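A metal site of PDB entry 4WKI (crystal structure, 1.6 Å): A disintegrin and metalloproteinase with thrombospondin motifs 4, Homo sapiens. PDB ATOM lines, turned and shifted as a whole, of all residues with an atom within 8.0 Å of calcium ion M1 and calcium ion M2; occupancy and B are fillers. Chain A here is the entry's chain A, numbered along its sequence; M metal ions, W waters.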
ATOM      1  N   PHE A   7     -24.280 -25.911   2.298  1.00  0.00           N
ATOM      2  CA  PHE A   7     -24.907 -26.581   3.444  1.00  0.00           C
ATOM      3  C   PHE A   7     -24.606 -25.812   4.725  1.00  0.00           C
ATOM      4  O   PHE A   7     -23.448 -25.588   5.088  1.00  0.00           O
ATOM      5  CB  PHE A   7     -24.348 -28.005   3.590  1.00  0.00           C
ATOM      6  CG  PHE A   7     -24.372 -28.784   2.310  1.00  0.00           C
ATOM      7  CD1 PHE A   7     -23.268 -28.768   1.457  1.00  0.00           C
ATOM      8  CD2 PHE A   7     -25.493 -29.490   1.939  1.00  0.00           C
ATOM      9  CE1 PHE A   7     -23.289 -29.466   0.261  1.00  0.00           C
ATOM     10  CE2 PHE A   7     -25.520 -30.201   0.742  1.00  0.00           C
ATOM     11  CZ  PHE A   7     -24.414 -30.178  -0.082  1.00  0.00           C
ATOM     12  N   VAL A   8     -25.657 -25.427   5.439  1.00  0.00           N
ATOM     13  CA  VAL A   8     -25.492 -24.712   6.700  1.00  0.00           C
ATOM     14  C   VAL A   8     -25.733 -25.719   7.802  1.00  0.00           C
ATOM     15  O   VAL A   8     -26.869 -26.142   8.030  1.00  0.00           O
ATOM     16  CB  VAL A   8     -26.495 -23.563   6.872  1.00  0.00           C
ATOM     17  CG1 VAL A   8     -26.185 -22.766   8.129  1.00  0.00           C
ATOM     18  CG2 VAL A   8     -26.524 -22.655   5.653  1.00  0.00           C
ATOM     19  N   GLU A   9     -24.649 -26.139   8.452  1.00  0.00           N
ATOM     20  CA  GLU A   9     -24.735 -27.061   9.570  1.00  0.00           C
ATOM     21  C   GLU A   9     -25.249 -26.332  10.809  1.00  0.00           C
ATOM     22  O   GLU A   9     -24.579 -25.466  11.382  1.00  0.00           O
ATOM     23  CB  GLU A   9     -23.385 -27.722   9.825  1.00  0.00           C
ATOM     24  CG  GLU A   9     -22.874 -28.545   8.645  1.00  0.00           C
ATOM     25  CD  GLU A   9     -21.431 -28.988   8.805  1.00  0.00           C
ATOM     26  OE1 GLU A   9     -20.539 -28.116   8.727  1.00  0.00           O
ATOM     27  OE2 GLU A   9     -21.141 -30.169   9.038  1.00  0.00           O
ATOM     28  N   THR A  10     -26.466 -26.694  11.222  1.00  0.00           N
ATOM     29  CA  THR A  10     -27.219 -25.870  12.167  1.00  0.00           C
ATOM     30  C   THR A  10     -27.392 -26.520  13.533  1.00  0.00           C
ATOM     31  O   THR A  10     -27.884 -27.637  13.660  1.00  0.00           O
ATOM     32  CB  THR A  10     -28.598 -25.473  11.586  1.00  0.00           C
ATOM     33  OG1 THR A  10     -28.443 -24.894  10.274  1.00  0.00           O
ATOM     34  CG2 THR A  10     -29.285 -24.453  12.503  1.00  0.00           C
ATOM     35  N   THR A  55     -28.030 -30.294  12.357  1.00  0.00           N
ATOM     36  CA  THR A  55     -26.996 -31.297  12.732  1.00  0.00           C
ATOM     37  C   THR A  55     -26.899 -31.561  14.249  1.00  0.00           C
ATOM     38  O   THR A  55     -26.422 -32.631  14.686  1.00  0.00           O
ATOM     39  CB  THR A  55     -25.622 -30.900  12.178  1.00  0.00           C
ATOM     40  OG1 THR A  55     -25.257 -29.598  12.675  1.00  0.00           O
ATOM     41  CG2 THR A  55     -25.669 -30.853  10.668  1.00  0.00           C
ATOM     42  N   THR A  89     -16.711 -26.547  18.036  1.00  0.00           N
ATOM     43  CA  THR A  89     -15.320 -26.989  17.954  1.00  0.00           C
ATOM     44  C   THR A  89     -14.571 -26.063  17.001  1.00  0.00           C
ATOM     45  O   THR A  89     -15.183 -25.377  16.181  1.00  0.00           O
ATOM     46  CB  THR A  89     -15.247 -28.445  17.484  1.00  0.00           C
ATOM     47  OG1 THR A  89     -15.821 -28.569  16.186  1.00  0.00           O
ATOM     48  CG2 THR A  89     -15.983 -29.355  18.474  1.00  0.00           C
ATOM     49  N   GLU A  91     -12.576 -26.501  14.322  1.00  0.00           N
ATOM     50  CA  GLU A  91     -12.489 -26.805  12.899  1.00  0.00           C
ATOM     51  C   GLU A  91     -13.760 -27.453  12.349  1.00  0.00           C
ATOM     52  O   GLU A  91     -14.355 -28.330  12.994  1.00  0.00           O
ATOM     53  CB  GLU A  91     -11.288 -27.715  12.635  1.00  0.00           C
ATOM     54  CG  GLU A  91      -9.978 -27.178  13.189  1.00  0.00           C
ATOM     55  CD  GLU A  91      -9.582 -25.846  12.578  1.00  0.00           C
ATOM     56  OE1 GLU A  91     -10.058 -25.524  11.461  1.00  0.00           O
ATOM     57  OE2 GLU A  91      -8.783 -25.118  13.193  1.00  0.00           O
ATOM     58  N   ASP A  92     -14.121 -27.016  11.143  1.00  0.00           N
ATOM     59  CA  ASP A  92     -15.328 -27.478  10.441  1.00  0.00           C
ATOM     60  C   ASP A  92     -15.248 -28.955  10.051  1.00  0.00           C
ATOM     61  O   ASP A  92     -16.283 -29.604   9.835  1.00  0.00           O
ATOM     62  CB  ASP A  92     -15.595 -26.625   9.204  1.00  0.00           C
ATOM     63  CG  ASP A  92     -17.063 -26.537   8.854  1.00  0.00           C
ATOM     64  OD1 ASP A  92     -17.867 -27.287   9.464  1.00  0.00           O
ATOM     65  OD2 ASP A  92     -17.400 -25.757   7.957  1.00  0.00           O
ATOM     66  N   SER A  93     -14.016 -29.465   9.963  1.00  0.00           N
ATOM     67  CA  SER A  93     -13.720 -30.891   9.769  1.00  0.00           C
ATOM     68  C   SER A  93     -14.312 -31.815  10.838  1.00  0.00           C
ATOM     69  O   SER A  93     -14.593 -32.968  10.563  1.00  0.00           O
ATOM     70  CB  SER A  93     -12.186 -31.128   9.735  1.00  0.00           C
ATOM     71  OG  SER A  93     -11.656 -31.265  11.058  1.00  0.00           O
ATOM     72  N   ASP A  94     -14.458 -31.299  12.057  1.00  0.00           N
ATOM     73  CA  ASP A  94     -15.032 -32.053  13.167  1.00  0.00           C
ATOM     74  C   ASP A  94     -16.537 -32.210  12.979  1.00  0.00           C
ATOM     75  O   ASP A  94     -17.206 -31.221  12.706  1.00  0.00           O
ATOM     76  CB  ASP A  94     -14.801 -31.260  14.460  1.00  0.00           C
ATOM     77  CG  ASP A  94     -15.013 -32.075  15.710  1.00  0.00           C
ATOM     78  OD1 ASP A  94     -14.169 -31.960  16.623  1.00  0.00           O
ATOM     79  OD2 ASP A  94     -16.019 -32.826  15.821  1.00  0.00           O
ATOM     80  N   PRO A  95     -17.089 -33.441  13.135  1.00  0.00           N
ATOM     81  CA  PRO A  95     -18.548 -33.651  12.996  1.00  0.00           C
ATOM     82  C   PRO A  95     -19.431 -32.815  13.930  1.00  0.00           C
ATOM     83  O   PRO A  95     -20.579 -32.514  13.582  1.00  0.00           O
ATOM     84  CB  PRO A  95     -18.747 -35.148  13.299  1.00  0.00           C
ATOM     85  CG  PRO A  95     -17.403 -35.780  13.219  1.00  0.00           C
ATOM     86  CD  PRO A  95     -16.341 -34.710  13.271  1.00  0.00           C
ATOM     87  N   ASP A  96     -18.920 -32.487  15.119  1.00  0.00           N
ATOM     88  CA  ASP A  96     -19.664 -31.700  16.109  1.00  0.00           C
ATOM     89  C   ASP A  96     -19.677 -30.221  15.757  1.00  0.00           C
ATOM     90  O   ASP A  96     -20.434 -29.447  16.361  1.00  0.00           O
ATOM     91  CB  ASP A  96     -19.044 -31.856  17.501  1.00  0.00           C
ATOM     92  CG  ASP A  96     -19.289 -33.217  18.098  1.00  0.00           C
ATOM     93  OD1 ASP A  96     -20.133 -33.974  17.576  1.00  0.00           O
ATOM     94  OD2 ASP A  96     -18.634 -33.525  19.116  1.00  0.00           O
ATOM     95  N   HIS A  97     -18.837 -29.804  14.821  1.00  0.00           N
ATOM     96  CA  HIS A  97     -18.807 -28.390  14.434  1.00  0.00           C
ATOM     97  C   HIS A  97     -20.096 -27.999  13.736  1.00  0.00           C
ATOM     98  O   HIS A  97     -20.647 -28.765  12.958  1.00  0.00           O
ATOM     99  CB  HIS A  97     -17.639 -28.067  13.504  1.00  0.00           C
ATOM    100  CG  HIS A  97     -17.504 -26.604  13.213  1.00  0.00           C
ATOM    101  ND1 HIS A  97     -16.788 -25.751  14.028  1.00  0.00           N
ATOM    102  CD2 HIS A  97     -17.997 -25.842  12.206  1.00  0.00           C
ATOM    103  CE1 HIS A  97     -16.856 -24.523  13.537  1.00  0.00           C
ATOM    104  NE2 HIS A  97     -17.566 -24.553  12.428  1.00  0.00           N
ATOM    105  N   PHE A  98     -20.558 -26.789  14.032  1.00  0.00           N
ATOM    106  CA  PHE A  98     -21.729 -26.236  13.385  1.00  0.00           C
ATOM    107  C   PHE A  98     -21.452 -24.823  12.891  1.00  0.00           C
ATOM    108  O   PHE A  98     -20.584 -24.109  13.457  1.00  0.00           O
ATOM    109  CB  PHE A  98     -22.953 -26.278  14.338  1.00  0.00           C
ATOM    110  CG  PHE A  98     -22.717 -25.629  15.678  1.00  0.00           C
ATOM    111  CD1 PHE A  98     -22.941 -24.274  15.838  1.00  0.00           C
ATOM    112  CD2 PHE A  98     -22.295 -26.377  16.775  1.00  0.00           C
ATOM    113  CE1 PHE A  98     -22.715 -23.671  17.072  1.00  0.00           C
ATOM    114  CE2 PHE A  98     -22.076 -25.779  18.014  1.00  0.00           C
ATOM    115  CZ  PHE A  98     -22.290 -24.412  18.158  1.00  0.00           C
ATOM    116  N   ASP A  99     -22.173 -24.453  11.843  1.00  0.00           N
ATOM    117  CA  ASP A  99     -21.991 -23.191  11.108  1.00  0.00           C
ATOM    118  C   ASP A  99     -22.861 -22.044  11.658  1.00  0.00           C
ATOM    119  O   ASP A  99     -22.507 -20.887  11.511  1.00  0.00           O
ATOM    120  CB  ASP A  99     -22.270 -23.380   9.611  1.00  0.00           C
ATOM    121  CG  ASP A  99     -21.362 -24.417   8.968  1.00  0.00           C
ATOM    122  OD1 ASP A  99     -20.161 -24.446   9.316  1.00  0.00           O
ATOM    123  OD2 ASP A  99     -21.853 -25.184   8.113  1.00  0.00           O
ATOM    124  N   THR A 100     -24.021 -22.367  12.229  1.00  0.00           N
ATOM    125  CA  THR A 100     -24.877 -21.337  12.802  1.00  0.00           C
ATOM    126  C   THR A 100     -25.670 -21.916  13.971  1.00  0.00           C
ATOM    127  O   THR A 100     -25.842 -23.139  14.078  1.00  0.00           O
ATOM    128  CB  THR A 100     -25.795 -20.690  11.729  1.00  0.00           C
ATOM    129  OG1 THR A 100     -26.224 -19.391  12.169  1.00  0.00           O
ATOM    130  CG2 THR A 100     -27.006 -21.576  11.426  1.00  0.00           C
ATOM    131  N   VAL A 126     -22.468 -15.561   8.963  1.00  0.00           N
ATOM    132  CA  VAL A 126     -22.719 -17.007   8.896  1.00  0.00           C
ATOM    133  C   VAL A 126     -21.485 -17.893   9.087  1.00  0.00           C
ATOM    134  O   VAL A 126     -21.588 -18.953   9.690  1.00  0.00           O
ATOM    135  CB  VAL A 126     -23.445 -17.412   7.595  1.00  0.00           C
ATOM    136  CG1 VAL A 126     -22.492 -17.449   6.411  1.00  0.00           C
ATOM    137  CG2 VAL A 126     -24.134 -18.774   7.743  1.00  0.00           C
ATOM    138  N   CYS A 127     -20.332 -17.452   8.596  1.00  0.00           N
ATOM    139  CA  CYS A 127     -19.099 -18.250   8.716  1.00  0.00           C
ATOM    140  C   CYS A 127     -18.128 -17.779   9.817  1.00  0.00           C
ATOM    141  O   CYS A 127     -16.969 -18.239   9.918  1.00  0.00           O
ATOM    142  CB  CYS A 127     -18.435 -18.405   7.342  1.00  0.00           C
ATOM    143  SG  CYS A 127     -19.394 -19.593   6.362  1.00  0.00           S
ATOM    144  N   GLY A 209     -19.270 -17.327   2.579  1.00  0.00           N
ATOM    145  CA  GLY A 209     -19.879 -18.628   2.835  1.00  0.00           C
ATOM    146  C   GLY A 209     -18.909 -19.786   2.686  1.00  0.00           C
ATOM    147  O   GLY A 209     -19.312 -20.907   2.388  1.00  0.00           O
ATOM    148  N   HIS A 210     -17.628 -19.521   2.925  1.00  0.00           N
ATOM    149  CA  HIS A 210     -16.562 -20.514   2.792  1.00  0.00           C
ATOM    150  C   HIS A 210     -16.696 -21.727   3.723  1.00  0.00           C
ATOM    151  O   HIS A 210     -16.150 -22.781   3.435  1.00  0.00           O
ATOM    152  CB  HIS A 210     -15.207 -19.824   3.020  1.00  0.00           C
ATOM    153  CG  HIS A 210     -15.074 -19.214   4.387  1.00  0.00           C
ATOM    154  ND1 HIS A 210     -14.707 -19.946   5.496  1.00  0.00           N
ATOM    155  CD2 HIS A 210     -15.281 -17.946   4.823  1.00  0.00           C
ATOM    156  CE1 HIS A 210     -14.681 -19.153   6.550  1.00  0.00           C
ATOM    157  NE2 HIS A 210     -15.033 -17.939   6.177  1.00  0.00           N
ATOM    158  N   CYS A 211     -17.428 -21.570   4.828  1.00  0.00           N
ATOM    159  CA  CYS A 211     -17.662 -22.645   5.788  1.00  0.00           C
ATOM    160  C   CYS A 211     -18.903 -23.484   5.435  1.00  0.00           C
ATOM    161  O   CYS A 211     -19.245 -24.394   6.172  1.00  0.00           O
ATOM    162  CB  CYS A 211     -17.815 -22.070   7.186  1.00  0.00           C
ATOM    163  SG  CYS A 211     -19.417 -21.298   7.491  1.00  0.00           S
ATOM    164  N   LEU A 212     -19.561 -23.172   4.327  1.00  0.00           N
ATOM    165  CA  LEU A 212     -20.804 -23.846   3.933  1.00  0.00           C
ATOM    166  C   LEU A 212     -20.553 -24.896   2.859  1.00  0.00           C
ATOM    167  O   LEU A 212     -21.486 -25.384   2.247  1.00  0.00           O
ATOM    168  CB  LEU A 212     -21.824 -22.822   3.447  1.00  0.00           C
ATOM    169  CG  LEU A 212     -22.130 -21.682   4.426  1.00  0.00           C
ATOM    170  CD1 LEU A 212     -23.048 -20.676   3.768  1.00  0.00           C
ATOM    171  CD2 LEU A 212     -22.747 -22.213   5.700  1.00  0.00           C
ATOM    172  N   LEU A 213     -19.294 -25.251   2.637  1.00  0.00           N
ATOM    173  CA  LEU A 213     -18.969 -26.083   1.483  1.00  0.00           C
ATOM    174  C   LEU A 213     -18.870 -27.568   1.777  1.00  0.00           C
ATOM    175  O   LEU A 213     -18.996 -28.382   0.863  1.00  0.00           O
ATOM    176  CB  LEU A 213     -17.698 -25.566   0.805  1.00  0.00           C
ATOM    177  CG  LEU A 213     -17.897 -24.189   0.170  1.00  0.00           C
ATOM    178  CD1 LEU A 213     -16.576 -23.653  -0.339  1.00  0.00           C
ATOM    179  CD2 LEU A 213     -18.937 -24.255  -0.942  1.00  0.00           C
ATOM    180  N   ASP A 214     -18.654 -27.917   3.042  1.00  0.00           N
ATOM    181  CA  ASP A 214     -18.592 -29.311   3.470  1.00  0.00           C
ATOM    182  C   ASP A 214     -20.004 -29.875   3.731  1.00  0.00           C
ATOM    183  O   ASP A 214     -20.911 -29.165   4.147  1.00  0.00           O
ATOM    184  CB  ASP A 214     -17.666 -29.484   4.686  1.00  0.00           C
ATOM    185  CG  ASP A 214     -18.124 -28.718   5.922  1.00  0.00           C
ATOM    186  OD1 ASP A 214     -18.507 -27.538   5.817  1.00  0.00           O
ATOM    187  OD2 ASP A 214     -18.036 -29.314   7.015  1.00  0.00           O
ATOM    188  N   LYS A 215     -20.173 -31.155   3.434  1.00  0.00           N
ATOM    189  CA  LYS A 215     -21.484 -31.767   3.513  1.00  0.00           C
ATOM    190  C   LYS A 215     -21.634 -32.419   4.872  1.00  0.00           C
ATOM    191  O   LYS A 215     -20.762 -33.164   5.308  1.00  0.00           O
ATOM    192  CB  LYS A 215     -21.666 -32.797   2.381  1.00  0.00           C
ATOM    193  CG  LYS A 215     -23.111 -33.070   2.030  1.00  0.00           C
ATOM    194  CD  LYS A 215     -23.214 -33.954   0.798  1.00  0.00           C
ATOM    195  CE  LYS A 215     -24.602 -34.570   0.653  1.00  0.00           C
ATOM    196  NZ  LYS A 215     -25.513 -33.770  -0.215  1.00  0.00           N
ATOM    197  N   PRO A 216     -22.746 -32.123   5.573  1.00  0.00           N
ATOM    198  CA  PRO A 216     -22.901 -32.756   6.876  1.00  0.00           C
ATOM    199  C   PRO A 216     -23.005 -34.284   6.805  1.00  0.00           C
ATOM    200  O   PRO A 216     -23.534 -34.852   5.858  1.00  0.00           O
ATOM    201  CB  PRO A 216     -24.183 -32.145   7.437  1.00  0.00           C
ATOM    202  CG  PRO A 216     -24.885 -31.548   6.290  1.00  0.00           C
ATOM    203  CD  PRO A 216     -23.844 -31.195   5.260  1.00  0.00           C
ATOM    204  N   GLU A 217     -22.543 -34.886   7.889  1.00  0.00           N
ATOM    205  CA  GLU A 217     -22.411 -36.313   8.098  1.00  0.00           C
ATOM    206  C   GLU A 217     -23.767 -36.973   8.383  1.00  0.00           C
ATOM    207  O   GLU A 217     -24.219 -37.903   7.702  1.00  0.00           O
ATOM    208  CB  GLU A 217     -21.498 -36.465   9.333  1.00  0.00           C
ATOM    209  CG  GLU A 217     -20.989 -37.857   9.669  1.00  0.00           C
ATOM    210  CD  GLU A 217     -19.468 -37.911   9.678  1.00  0.00           C
ATOM    211  OE1 GLU A 217     -18.891 -38.155  10.759  1.00  0.00           O
ATOM    212  OE2 GLU A 217     -18.862 -37.693   8.611  1.00  0.00           O
HETATM  213 CA    CA M   1     -18.673 -29.597   9.068  1.00  0.00          CA
HETATM  214 CA    CA M   2     -19.712 -26.255   7.559  1.00  0.00          CA
HETATM  215  O   HOH W   1     -21.302 -26.953   5.843  1.00  0.00           O
HETATM  216  O   HOH W   2     -19.206 -30.233  11.220  1.00  0.00           O
HETATM  217  O   HOH W   3     -18.513 -31.886   8.422  1.00  0.00           O
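The backbone NH (N) of Thr 100 sits at hydrogen-bond distance from the backbone carbonyl oxygen (O) of Glu 9.
The side-chain sulfur (SG) of Cys 211 is disulfide-bonded to the side-chain sulfur (SG) of Cys 127.
Of the 27 residues printed, 3 come within 4 Å of calcium ion M1.
Five residues have an atom within 4 Å of calcium ion M2: Glu 9, Asp 92, Asp 99, Cys 211 and Asp 214.
The nearest printed residue that does not touch calcium ion M2 is Leu 212 (4.5 Å).
Calcium ion M1 is bound by OD2 of Asp 214 (2.2 Å), water W2 (2.3 Å), water W3 (2.4 Å), OE1 of Glu 9 (2.4 Å), OD1 of Asp 92 (2.5 Å), O of Asp 92 (2.5 Å) and OE2 of Glu 9 (2.5 Å).
Calcium ion M1 has seven donor atoms within binding distance.
Calcium ion M2 is bound by OE1 of Glu 9 (2.3 Å), O of Cys 211 (2.4 Å), OD2 of Asp 92 (2.4 Å), water W1 (2.4 Å), OD2 of Asp 99 (2.5 Å), OD1 of Asp 214 (2.5 Å), OD1 of Asp 99 (2.6 Å) and OD1 of Asp 92 (2.8 Å).
Water W1 bridges O of Phe 7 (2.7 Å) and O of Asp 214 (2.8 Å).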
